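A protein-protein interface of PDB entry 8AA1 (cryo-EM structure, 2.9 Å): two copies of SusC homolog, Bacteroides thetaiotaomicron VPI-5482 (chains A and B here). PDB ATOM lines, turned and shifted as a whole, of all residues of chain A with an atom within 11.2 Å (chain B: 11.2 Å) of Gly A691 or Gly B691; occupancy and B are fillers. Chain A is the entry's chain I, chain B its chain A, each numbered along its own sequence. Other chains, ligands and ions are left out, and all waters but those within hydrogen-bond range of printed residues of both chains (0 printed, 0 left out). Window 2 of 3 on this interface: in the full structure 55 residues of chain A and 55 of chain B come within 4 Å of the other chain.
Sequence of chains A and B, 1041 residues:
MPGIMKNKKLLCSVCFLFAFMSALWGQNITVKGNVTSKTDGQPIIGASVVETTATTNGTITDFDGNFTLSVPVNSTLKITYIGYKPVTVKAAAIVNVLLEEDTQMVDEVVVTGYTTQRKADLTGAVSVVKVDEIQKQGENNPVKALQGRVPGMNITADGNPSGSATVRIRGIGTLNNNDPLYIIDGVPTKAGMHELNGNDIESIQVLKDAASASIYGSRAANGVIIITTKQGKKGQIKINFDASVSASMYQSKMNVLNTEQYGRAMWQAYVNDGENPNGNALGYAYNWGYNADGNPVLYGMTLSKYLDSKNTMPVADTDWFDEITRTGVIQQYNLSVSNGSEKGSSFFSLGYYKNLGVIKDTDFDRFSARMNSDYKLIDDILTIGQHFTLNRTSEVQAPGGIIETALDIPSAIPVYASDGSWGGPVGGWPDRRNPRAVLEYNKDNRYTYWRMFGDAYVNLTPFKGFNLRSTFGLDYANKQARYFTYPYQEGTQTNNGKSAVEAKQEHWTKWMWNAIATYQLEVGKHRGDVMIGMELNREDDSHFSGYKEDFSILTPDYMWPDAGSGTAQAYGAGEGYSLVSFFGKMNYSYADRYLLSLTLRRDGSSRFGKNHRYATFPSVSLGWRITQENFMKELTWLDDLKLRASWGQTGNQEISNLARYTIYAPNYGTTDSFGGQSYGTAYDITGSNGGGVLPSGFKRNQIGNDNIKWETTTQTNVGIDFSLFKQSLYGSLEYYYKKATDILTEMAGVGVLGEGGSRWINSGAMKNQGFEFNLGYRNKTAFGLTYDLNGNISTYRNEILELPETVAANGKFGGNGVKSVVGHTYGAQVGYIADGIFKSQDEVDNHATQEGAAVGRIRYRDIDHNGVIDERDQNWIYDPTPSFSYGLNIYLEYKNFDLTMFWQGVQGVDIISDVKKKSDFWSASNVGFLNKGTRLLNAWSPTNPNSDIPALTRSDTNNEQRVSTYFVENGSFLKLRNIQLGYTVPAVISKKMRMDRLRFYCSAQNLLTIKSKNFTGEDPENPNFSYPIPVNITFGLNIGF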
ATOM      1  N   THR A 567      25.302  19.585 -11.992  1.00  0.00           N
ATOM      2  CA  THR A 567      26.598  20.245 -12.041  1.00  0.00           C
ATOM      3  C   THR A 567      27.451  19.836 -10.847  1.00  0.00           C
ATOM      4  O   THR A 567      26.965  19.739  -9.717  1.00  0.00           O
ATOM      5  CB  THR A 567      26.418  21.764 -12.062  1.00  0.00           C
ATOM      6  OG1 THR A 567      25.475  22.118 -13.080  1.00  0.00           O
ATOM      7  CG2 THR A 567      27.742  22.456 -12.350  1.00  0.00           C
ATOM      8  N   TYR A 668      37.473  31.618 -10.136  1.00  0.00           N
ATOM      9  CA  TYR A 668      36.497  31.458 -11.208  1.00  0.00           C
ATOM     10  C   TYR A 668      35.082  31.763 -10.734  1.00  0.00           C
ATOM     11  O   TYR A 668      34.219  32.115 -11.546  1.00  0.00           O
ATOM     12  CB  TYR A 668      36.576  30.040 -11.775  1.00  0.00           C
ATOM     13  CG  TYR A 668      35.805  29.839 -13.061  1.00  0.00           C
ATOM     14  CD1 TYR A 668      36.379  30.131 -14.290  1.00  0.00           C
ATOM     15  CD2 TYR A 668      34.507  29.349 -13.044  1.00  0.00           C
ATOM     16  CE1 TYR A 668      35.679  29.945 -15.466  1.00  0.00           C
ATOM     17  CE2 TYR A 668      33.800  29.160 -14.215  1.00  0.00           C
ATOM     18  CZ  TYR A 668      34.390  29.461 -15.423  1.00  0.00           C
ATOM     19  OH  TYR A 668      33.688  29.274 -16.590  1.00  0.00           O
ATOM     20  N   ALA A 682      35.052  35.399 -14.218  1.00  0.00           N
ATOM     21  CA  ALA A 682      34.520  34.653 -15.355  1.00  0.00           C
ATOM     22  C   ALA A 682      33.474  35.524 -16.027  1.00  0.00           C
ATOM     23  O   ALA A 682      32.452  35.843 -15.412  1.00  0.00           O
ATOM     24  CB  ALA A 682      33.917  33.322 -14.912  1.00  0.00           C
ATOM     25  N   TYR A 683      33.722  35.910 -17.273  1.00  0.00           N
ATOM     26  CA  TYR A 683      32.827  36.802 -17.994  1.00  0.00           C
ATOM     27  C   TYR A 683      32.515  36.225 -19.366  1.00  0.00           C
ATOM     28  O   TYR A 683      33.405  35.718 -20.054  1.00  0.00           O
ATOM     29  CB  TYR A 683      33.436  38.200 -18.136  1.00  0.00           C
ATOM     30  CG  TYR A 683      32.453  39.253 -18.590  1.00  0.00           C
ATOM     31  CD1 TYR A 683      31.599  39.865 -17.684  1.00  0.00           C
ATOM     32  CD2 TYR A 683      32.385  39.639 -19.920  1.00  0.00           C
ATOM     33  CE1 TYR A 683      30.700  40.829 -18.092  1.00  0.00           C
ATOM     34  CE2 TYR A 683      31.489  40.602 -20.337  1.00  0.00           C
ATOM     35  CZ  TYR A 683      30.649  41.194 -19.419  1.00  0.00           C
ATOM     36  OH  TYR A 683      29.755  42.154 -19.830  1.00  0.00           O
ATOM     37  N   ASP A 684      31.243  36.307 -19.755  1.00  0.00           N
ATOM     38  CA  ASP A 684      30.800  35.869 -21.078  1.00  0.00           C
ATOM     39  C   ASP A 684      31.142  36.971 -22.075  1.00  0.00           C
ATOM     40  O   ASP A 684      30.300  37.770 -22.491  1.00  0.00           O
ATOM     41  CB  ASP A 684      29.309  35.555 -21.069  1.00  0.00           C
ATOM     42  CG  ASP A 684      28.842  34.909 -22.357  1.00  0.00           C
ATOM     43  OD1 ASP A 684      29.702  34.518 -23.173  1.00  0.00           O
ATOM     44  OD2 ASP A 684      27.614  34.794 -22.552  1.00  0.00           O
ATOM     45  N   ILE A 685      32.418  37.009 -22.462  1.00  0.00           N
ATOM     46  CA  ILE A 685      32.894  38.077 -23.335  1.00  0.00           C
ATOM     47  C   ILE A 685      32.274  37.967 -24.723  1.00  0.00           C
ATOM     48  O   ILE A 685      32.099  38.979 -25.412  1.00  0.00           O
ATOM     49  CB  ILE A 685      34.434  38.073 -23.389  1.00  0.00           C
ATOM     50  CG1 ILE A 685      34.951  39.410 -23.922  1.00  0.00           C
ATOM     51  CG2 ILE A 685      34.954  36.913 -24.225  1.00  0.00           C
ATOM     52  CD1 ILE A 685      34.602  40.586 -23.040  1.00  0.00           C
ATOM     53  N   THR A 686      31.927  36.754 -25.159  1.00  0.00           N
ATOM     54  CA  THR A 686      31.310  36.588 -26.470  1.00  0.00           C
ATOM     55  C   THR A 686      29.846  37.008 -26.472  1.00  0.00           C
ATOM     56  O   THR A 686      29.362  37.543 -27.475  1.00  0.00           O
ATOM     57  CB  THR A 686      31.436  35.136 -26.934  1.00  0.00           C
ATOM     58  OG1 THR A 686      30.812  34.271 -25.977  1.00  0.00           O
ATOM     59  CG2 THR A 686      32.899  34.751 -27.079  1.00  0.00           C
ATOM     60  N   GLY A 687      29.131  36.778 -25.374  1.00  0.00           N
ATOM     61  CA  GLY A 687      27.734  37.154 -25.289  1.00  0.00           C
ATOM     62  C   GLY A 687      26.794  36.076 -25.785  1.00  0.00           C
ATOM     63  O   GLY A 687      25.897  36.347 -26.589  1.00  0.00           O
ATOM     64  N   SER A 688      26.989  34.844 -25.312  1.00  0.00           N
ATOM     65  CA  SER A 688      26.173  33.708 -25.723  1.00  0.00           C
ATOM     66  C   SER A 688      25.366  33.130 -24.566  1.00  0.00           C
ATOM     67  O   SER A 688      24.871  32.002 -24.667  1.00  0.00           O
ATOM     68  CB  SER A 688      27.048  32.624 -26.352  1.00  0.00           C
ATOM     69  OG  SER A 688      28.028  32.168 -25.437  1.00  0.00           O
ATOM     70  N   ASN A 689      25.220  33.882 -23.472  1.00  0.00           N
ATOM     71  CA  ASN A 689      24.502  33.424 -22.280  1.00  0.00           C
ATOM     72  C   ASN A 689      25.068  32.105 -21.759  1.00  0.00           C
ATOM     73  O   ASN A 689      24.328  31.207 -21.352  1.00  0.00           O
ATOM     74  CB  ASN A 689      23.000  33.301 -22.547  1.00  0.00           C
ATOM     75  CG  ASN A 689      22.320  34.646 -22.680  1.00  0.00           C
ATOM     76  OD1 ASN A 689      21.775  34.976 -23.733  1.00  0.00           O
ATOM     77  ND2 ASN A 689      22.346  35.432 -21.611  1.00  0.00           N
ATOM     78  N   GLY A 690      26.394  31.987 -21.770  1.00  0.00           N
ATOM     79  CA  GLY A 690      27.029  30.790 -21.258  1.00  0.00           C
ATOM     80  C   GLY A 690      26.939  29.624 -22.230  1.00  0.00           C
ATOM     81  O   GLY A 690      26.929  29.792 -23.450  1.00  0.00           O
ATOM     82  N   GLY A 691      26.872  28.422 -21.667  1.00  0.00           N
ATOM     83  CA  GLY A 691      26.853  27.206 -22.449  1.00  0.00           C
ATOM     84  C   GLY A 691      28.174  26.477 -22.540  1.00  0.00           C
ATOM     85  O   GLY A 691      28.259  25.478 -23.263  1.00  0.00           O
ATOM     86  N   GLY A 692      29.201  26.941 -21.836  1.00  0.00           N
ATOM     87  CA  GLY A 692      30.502  26.303 -21.864  1.00  0.00           C
ATOM     88  C   GLY A 692      31.405  26.798 -20.755  1.00  0.00           C
ATOM     89  O   GLY A 692      30.935  27.105 -19.657  1.00  0.00           O
ATOM     90  N   VAL A 693      32.702  26.880 -21.027  1.00  0.00           N
ATOM     91  CA  VAL A 693      33.677  27.378 -20.065  1.00  0.00           C
ATOM     92  C   VAL A 693      34.011  28.813 -20.449  1.00  0.00           C
ATOM     93  O   VAL A 693      34.587  29.065 -21.513  1.00  0.00           O
ATOM     94  CB  VAL A 693      34.935  26.502 -20.026  1.00  0.00           C
ATOM     95  CG1 VAL A 693      35.937  27.057 -19.028  1.00  0.00           C
ATOM     96  CG2 VAL A 693      34.569  25.068 -19.678  1.00  0.00           C
ATOM     97  N   LEU A 694      33.649  29.756 -19.585  1.00  0.00           N
ATOM     98  CA  LEU A 694      33.919  31.156 -19.857  1.00  0.00           C
ATOM     99  C   LEU A 694      35.401  31.463 -19.650  1.00  0.00           C
ATOM    100  O   LEU A 694      36.079  30.791 -18.868  1.00  0.00           O
ATOM    101  CB  LEU A 694      33.078  32.048 -18.950  1.00  0.00           C
ATOM    102  CG  LEU A 694      31.561  31.965 -19.106  1.00  0.00           C
ATOM    103  CD1 LEU A 694      30.888  33.019 -18.247  1.00  0.00           C
ATOM    104  CD2 LEU A 694      31.160  32.119 -20.562  1.00  0.00           C
ATOM    105  N   PRO A 695      35.932  32.465 -20.350  1.00  0.00           N
ATOM    106  CA  PRO A 695      37.303  32.905 -20.072  1.00  0.00           C
ATOM    107  C   PRO A 695      37.429  33.405 -18.641  1.00  0.00           C
ATOM    108  O   PRO A 695      36.519  34.036 -18.101  1.00  0.00           O
ATOM    109  CB  PRO A 695      37.527  34.031 -21.087  1.00  0.00           C
ATOM    110  CG  PRO A 695      36.536  33.770 -22.172  1.00  0.00           C
ATOM    111  CD  PRO A 695      35.341  33.182 -21.492  1.00  0.00           C
ATOM    112  N   THR B 567      36.202  22.519 -16.357  1.00  0.00           N
ATOM    113  CA  THR B 567      35.123  21.653 -15.904  1.00  0.00           C
ATOM    114  C   THR B 567      35.561  20.844 -14.689  1.00  0.00           C
ATOM    115  O   THR B 567      36.687  20.340 -14.630  1.00  0.00           O
ATOM    116  CB  THR B 567      34.686  20.715 -17.030  1.00  0.00           C
ATOM    117  OG1 THR B 567      34.445  21.477 -18.218  1.00  0.00           O
ATOM    118  CG2 THR B 567      33.413  19.976 -16.647  1.00  0.00           C
ATOM    119  N   TYR B 668      25.633   8.976 -15.228  1.00  0.00           N
ATOM    120  CA  TYR B 668      25.555  10.129 -16.118  1.00  0.00           C
ATOM    121  C   TYR B 668      26.664  10.112 -17.162  1.00  0.00           C
ATOM    122  O   TYR B 668      26.516  10.711 -18.233  1.00  0.00           O
ATOM    123  CB  TYR B 668      25.610  11.420 -15.303  1.00  0.00           C
ATOM    124  CG  TYR B 668      25.270  12.667 -16.086  1.00  0.00           C
ATOM    125  CD1 TYR B 668      23.953  13.075 -16.241  1.00  0.00           C
ATOM    126  CD2 TYR B 668      26.267  13.442 -16.662  1.00  0.00           C
ATOM    127  CE1 TYR B 668      23.638  14.216 -16.954  1.00  0.00           C
ATOM    128  CE2 TYR B 668      25.962  14.583 -17.377  1.00  0.00           C
ATOM    129  CZ  TYR B 668      24.647  14.966 -17.519  1.00  0.00           C
ATOM    130  OH  TYR B 668      24.340  16.102 -18.230  1.00  0.00           O
ATOM    131  N   ALA B 682      22.981   9.973 -20.594  1.00  0.00           N
ATOM    132  CA  ALA B 682      22.786  11.403 -20.810  1.00  0.00           C
ATOM    133  C   ALA B 682      22.668  11.629 -22.307  1.00  0.00           C
ATOM    134  O   ALA B 682      23.625  11.373 -23.045  1.00  0.00           O
ATOM    135  CB  ALA B 682      23.941  12.215 -20.228  1.00  0.00           C
ATOM    136  N   TYR B 683      21.510  12.101 -22.756  1.00  0.00           N
ATOM    137  CA  TYR B 683      21.256  12.291 -24.175  1.00  0.00           C
ATOM    138  C   TYR B 683      20.700  13.685 -24.419  1.00  0.00           C
ATOM    139  O   TYR B 683      19.842  14.162 -23.672  1.00  0.00           O
ATOM    140  CB  TYR B 683      20.284  11.235 -24.709  1.00  0.00           C
ATOM    141  CG  TYR B 683      20.214  11.174 -26.216  1.00  0.00           C
ATOM    142  CD1 TYR B 683      21.164  10.471 -26.945  1.00  0.00           C
ATOM    143  CD2 TYR B 683      19.196  11.811 -26.910  1.00  0.00           C
ATOM    144  CE1 TYR B 683      21.104  10.410 -28.321  1.00  0.00           C
ATOM    145  CE2 TYR B 683      19.129  11.755 -28.287  1.00  0.00           C
ATOM    146  CZ  TYR B 683      20.085  11.054 -28.987  1.00  0.00           C
ATOM    147  OH  TYR B 683      20.021  10.995 -30.359  1.00  0.00           O
ATOM    148  N   ASP B 684      21.199  14.332 -25.473  1.00  0.00           N
ATOM    149  CA  ASP B 684      20.710  15.647 -25.885  1.00  0.00           C
ATOM    150  C   ASP B 684      19.415  15.444 -26.664  1.00  0.00           C
ATOM    151  O   ASP B 684      19.371  15.478 -27.896  1.00  0.00           O
ATOM    152  CB  ASP B 684      21.761  16.377 -26.713  1.00  0.00           C
ATOM    153  CG  ASP B 684      21.385  17.816 -26.994  1.00  0.00           C
ATOM    154  OD1 ASP B 684      20.415  18.310 -26.383  1.00  0.00           O
ATOM    155  OD2 ASP B 684      22.059  18.453 -27.831  1.00  0.00           O
ATOM    156  N   ILE B 685      18.332  15.222 -25.915  1.00  0.00           N
ATOM    157  CA  ILE B 685      17.051  14.913 -26.541  1.00  0.00           C
ATOM    158  C   ILE B 685      16.513  16.114 -27.311  1.00  0.00           C
ATOM    159  O   ILE B 685      15.788  15.950 -28.299  1.00  0.00           O
ATOM    160  CB  ILE B 685      16.050  14.409 -25.484  1.00  0.00           C
ATOM    161  CG1 ILE B 685      14.886  13.683 -26.158  1.00  0.00           C
ATOM    162  CG2 ILE B 685      15.551  15.550 -24.609  1.00  0.00           C
ATOM    163  CD1 ILE B 685      15.304  12.443 -26.910  1.00  0.00           C
ATOM    164  N   THR B 686      16.854  17.333 -26.886  1.00  0.00           N
ATOM    165  CA  THR B 686      16.388  18.520 -27.594  1.00  0.00           C
ATOM    166  C   THR B 686      17.156  18.755 -28.887  1.00  0.00           C
ATOM    167  O   THR B 686      16.573  19.225 -29.870  1.00  0.00           O
ATOM    168  CB  THR B 686      16.497  19.751 -26.692  1.00  0.00           C
ATOM    169  OG1 THR B 686      17.858  19.922 -26.276  1.00  0.00           O
ATOM    170  CG2 THR B 686      15.615  19.589 -25.465  1.00  0.00           C
ATOM    171  N   GLY B 687      18.448  18.441 -28.909  1.00  0.00           N
ATOM    172  CA  GLY B 687      19.249  18.625 -30.102  1.00  0.00           C
ATOM    173  C   GLY B 687      19.873  20.001 -30.196  1.00  0.00           C
ATOM    174  O   GLY B 687      19.782  20.662 -31.235  1.00  0.00           O
ATOM    175  N   SER B 688      20.513  20.447 -29.114  1.00  0.00           N
ATOM    176  CA  SER B 688      21.138  21.762 -29.060  1.00  0.00           C
ATOM    177  C   SER B 688      22.653  21.675 -28.900  1.00  0.00           C
ATOM    178  O   SER B 688      23.289  22.670 -28.534  1.00  0.00           O
ATOM    179  CB  SER B 688      20.533  22.593 -27.926  1.00  0.00           C
ATOM    180  OG  SER B 688      20.717  21.954 -26.676  1.00  0.00           O
ATOM    181  N   ASN B 689      23.240  20.508 -29.171  1.00  0.00           N
ATOM    182  CA  ASN B 689      24.680  20.285 -29.018  1.00  0.00           C
ATOM    183  C   ASN B 689      25.151  20.627 -27.607  1.00  0.00           C
ATOM    184  O   ASN B 689      26.213  21.221 -27.413  1.00  0.00           O
ATOM    185  CB  ASN B 689      25.480  21.071 -30.060  1.00  0.00           C
ATOM    186  CG  ASN B 689      25.339  20.498 -31.455  1.00  0.00           C
ATOM    187  OD1 ASN B 689      24.832  21.159 -32.360  1.00  0.00           O
ATOM    188  ND2 ASN B 689      25.790  19.263 -31.636  1.00  0.00           N
ATOM    189  N   GLY B 690      24.355  20.248 -26.611  1.00  0.00           N
ATOM    190  CA  GLY B 690      24.733  20.488 -25.233  1.00  0.00           C
ATOM    191  C   GLY B 690      24.525  21.936 -24.818  1.00  0.00           C
ATOM    192  O   GLY B 690      23.623  22.627 -25.296  1.00  0.00           O
ATOM    193  N   GLY B 691      25.380  22.395 -23.911  1.00  0.00           N
ATOM    194  CA  GLY B 691      25.276  23.727 -23.359  1.00  0.00           C
ATOM    195  C   GLY B 691      24.641  23.810 -21.991  1.00  0.00           C
ATOM    196  O   GLY B 691      24.437  24.921 -21.491  1.00  0.00           O
ATOM    197  N   GLY B 692      24.324  22.676 -21.372  1.00  0.00           N
ATOM    198  CA  GLY B 692      23.714  22.665 -20.058  1.00  0.00           C
ATOM    199  C   GLY B 692      23.745  21.289 -19.426  1.00  0.00           C
ATOM    200  O   GLY B 692      24.696  20.530 -19.630  1.00  0.00           O
ATOM    201  N   VAL B 693      22.714  20.956 -18.659  1.00  0.00           N
ATOM    202  CA  VAL B 693      22.598  19.650 -18.023  1.00  0.00           C
ATOM    203  C   VAL B 693      21.616  18.825 -18.843  1.00  0.00           C
ATOM    204  O   VAL B 693      20.427  19.151 -18.922  1.00  0.00           O
ATOM    205  CB  VAL B 693      22.144  19.769 -16.562  1.00  0.00           C
ATOM    206  CG1 VAL B 693      22.016  18.391 -15.935  1.00  0.00           C
ATOM    207  CG2 VAL B 693      23.120  20.628 -15.775  1.00  0.00           C
ATOM    208  N   LEU B 694      22.113  17.756 -19.458  1.00  0.00           N
ATOM    209  CA  LEU B 694      21.261  16.903 -20.267  1.00  0.00           C
ATOM    210  C   LEU B 694      20.370  16.040 -19.376  1.00  0.00           C
ATOM    211  O   LEU B 694      20.725  15.738 -18.235  1.00  0.00           O
ATOM    212  CB  LEU B 694      22.106  16.007 -21.169  1.00  0.00           C
ATOM    213  CG  LEU B 694      22.977  16.699 -22.215  1.00  0.00           C
ATOM    214  CD1 LEU B 694      23.626  15.668 -23.119  1.00  0.00           C
ATOM    215  CD2 LEU B 694      22.162  17.691 -23.026  1.00  0.00           C
ATOM    216  N   PRO B 695      19.198  15.643 -19.871  1.00  0.00           N
ATOM    217  CA  PRO B 695      18.377  14.684 -19.124  1.00  0.00           C
ATOM    218  C   PRO B 695      19.117  13.367 -18.941  1.00  0.00           C
ATOM    219  O   PRO B 695      19.841  12.912 -19.828  1.00  0.00           O
ATOM    220  CB  PRO B 695      17.134  14.516 -20.005  1.00  0.00           C
ATOM    221  CG  PRO B 695      17.093  15.750 -20.844  1.00  0.00           C
ATOM    222  CD  PRO B 695      18.522  16.119 -21.089  1.00  0.00           C
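Among the printed residues, pairs that only touch across the chains: Gly A691 with Gly B691 (3.5 Å), Thr A567 with Val B693 (3.9 Å) and Val A693 with Thr B567 (3.9 Å).
Thr A567 touches Val B693, and with the chains exchanged Val A693 touches Thr B567. Gly B691 touches its own counterpart, Gly A691. Positions printed for both chains: 567, 668, 682, 683, 684, 685, 686, 687, 688, 689, 690, 691, 692, 693, 694 and 695.
Hydrophobic or aromatic side chains of chain A that line the printed part of chain B: Val A693. Hydrophobic or aromatic side chains of chain B within 4 Å of the printed part of chain A: Val B693. Among the printed residues, 3 pairs touch across the chains. Among the printed residues, no Asp or Glu carboxylate lies within 4 Å of a Lys or Arg side-chain nitrogen of the other chain.
Gly A691 touches just one residue of chain B: Gly B691. Gly B691 touches just one residue of chain A: Gly A691 (3.5 Å). No residue of chain B comes within 4 Å of Gly A690. No residue of chain A comes within 4 Å of Gly B690. Printed residues of chain A within 4 Å of Thr B567: Val A693. Of the printed residues of chain B, Thr A567 touches Val B693. Of the printed residues of chain B, Val A693 touches Thr B567 (3.9 Å). Of the printed residues of chain A, Val B693 touches Thr A567. The nearest printed residue of chain B that does not touch Thr A567 is Gly B692 (6.6 Å).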
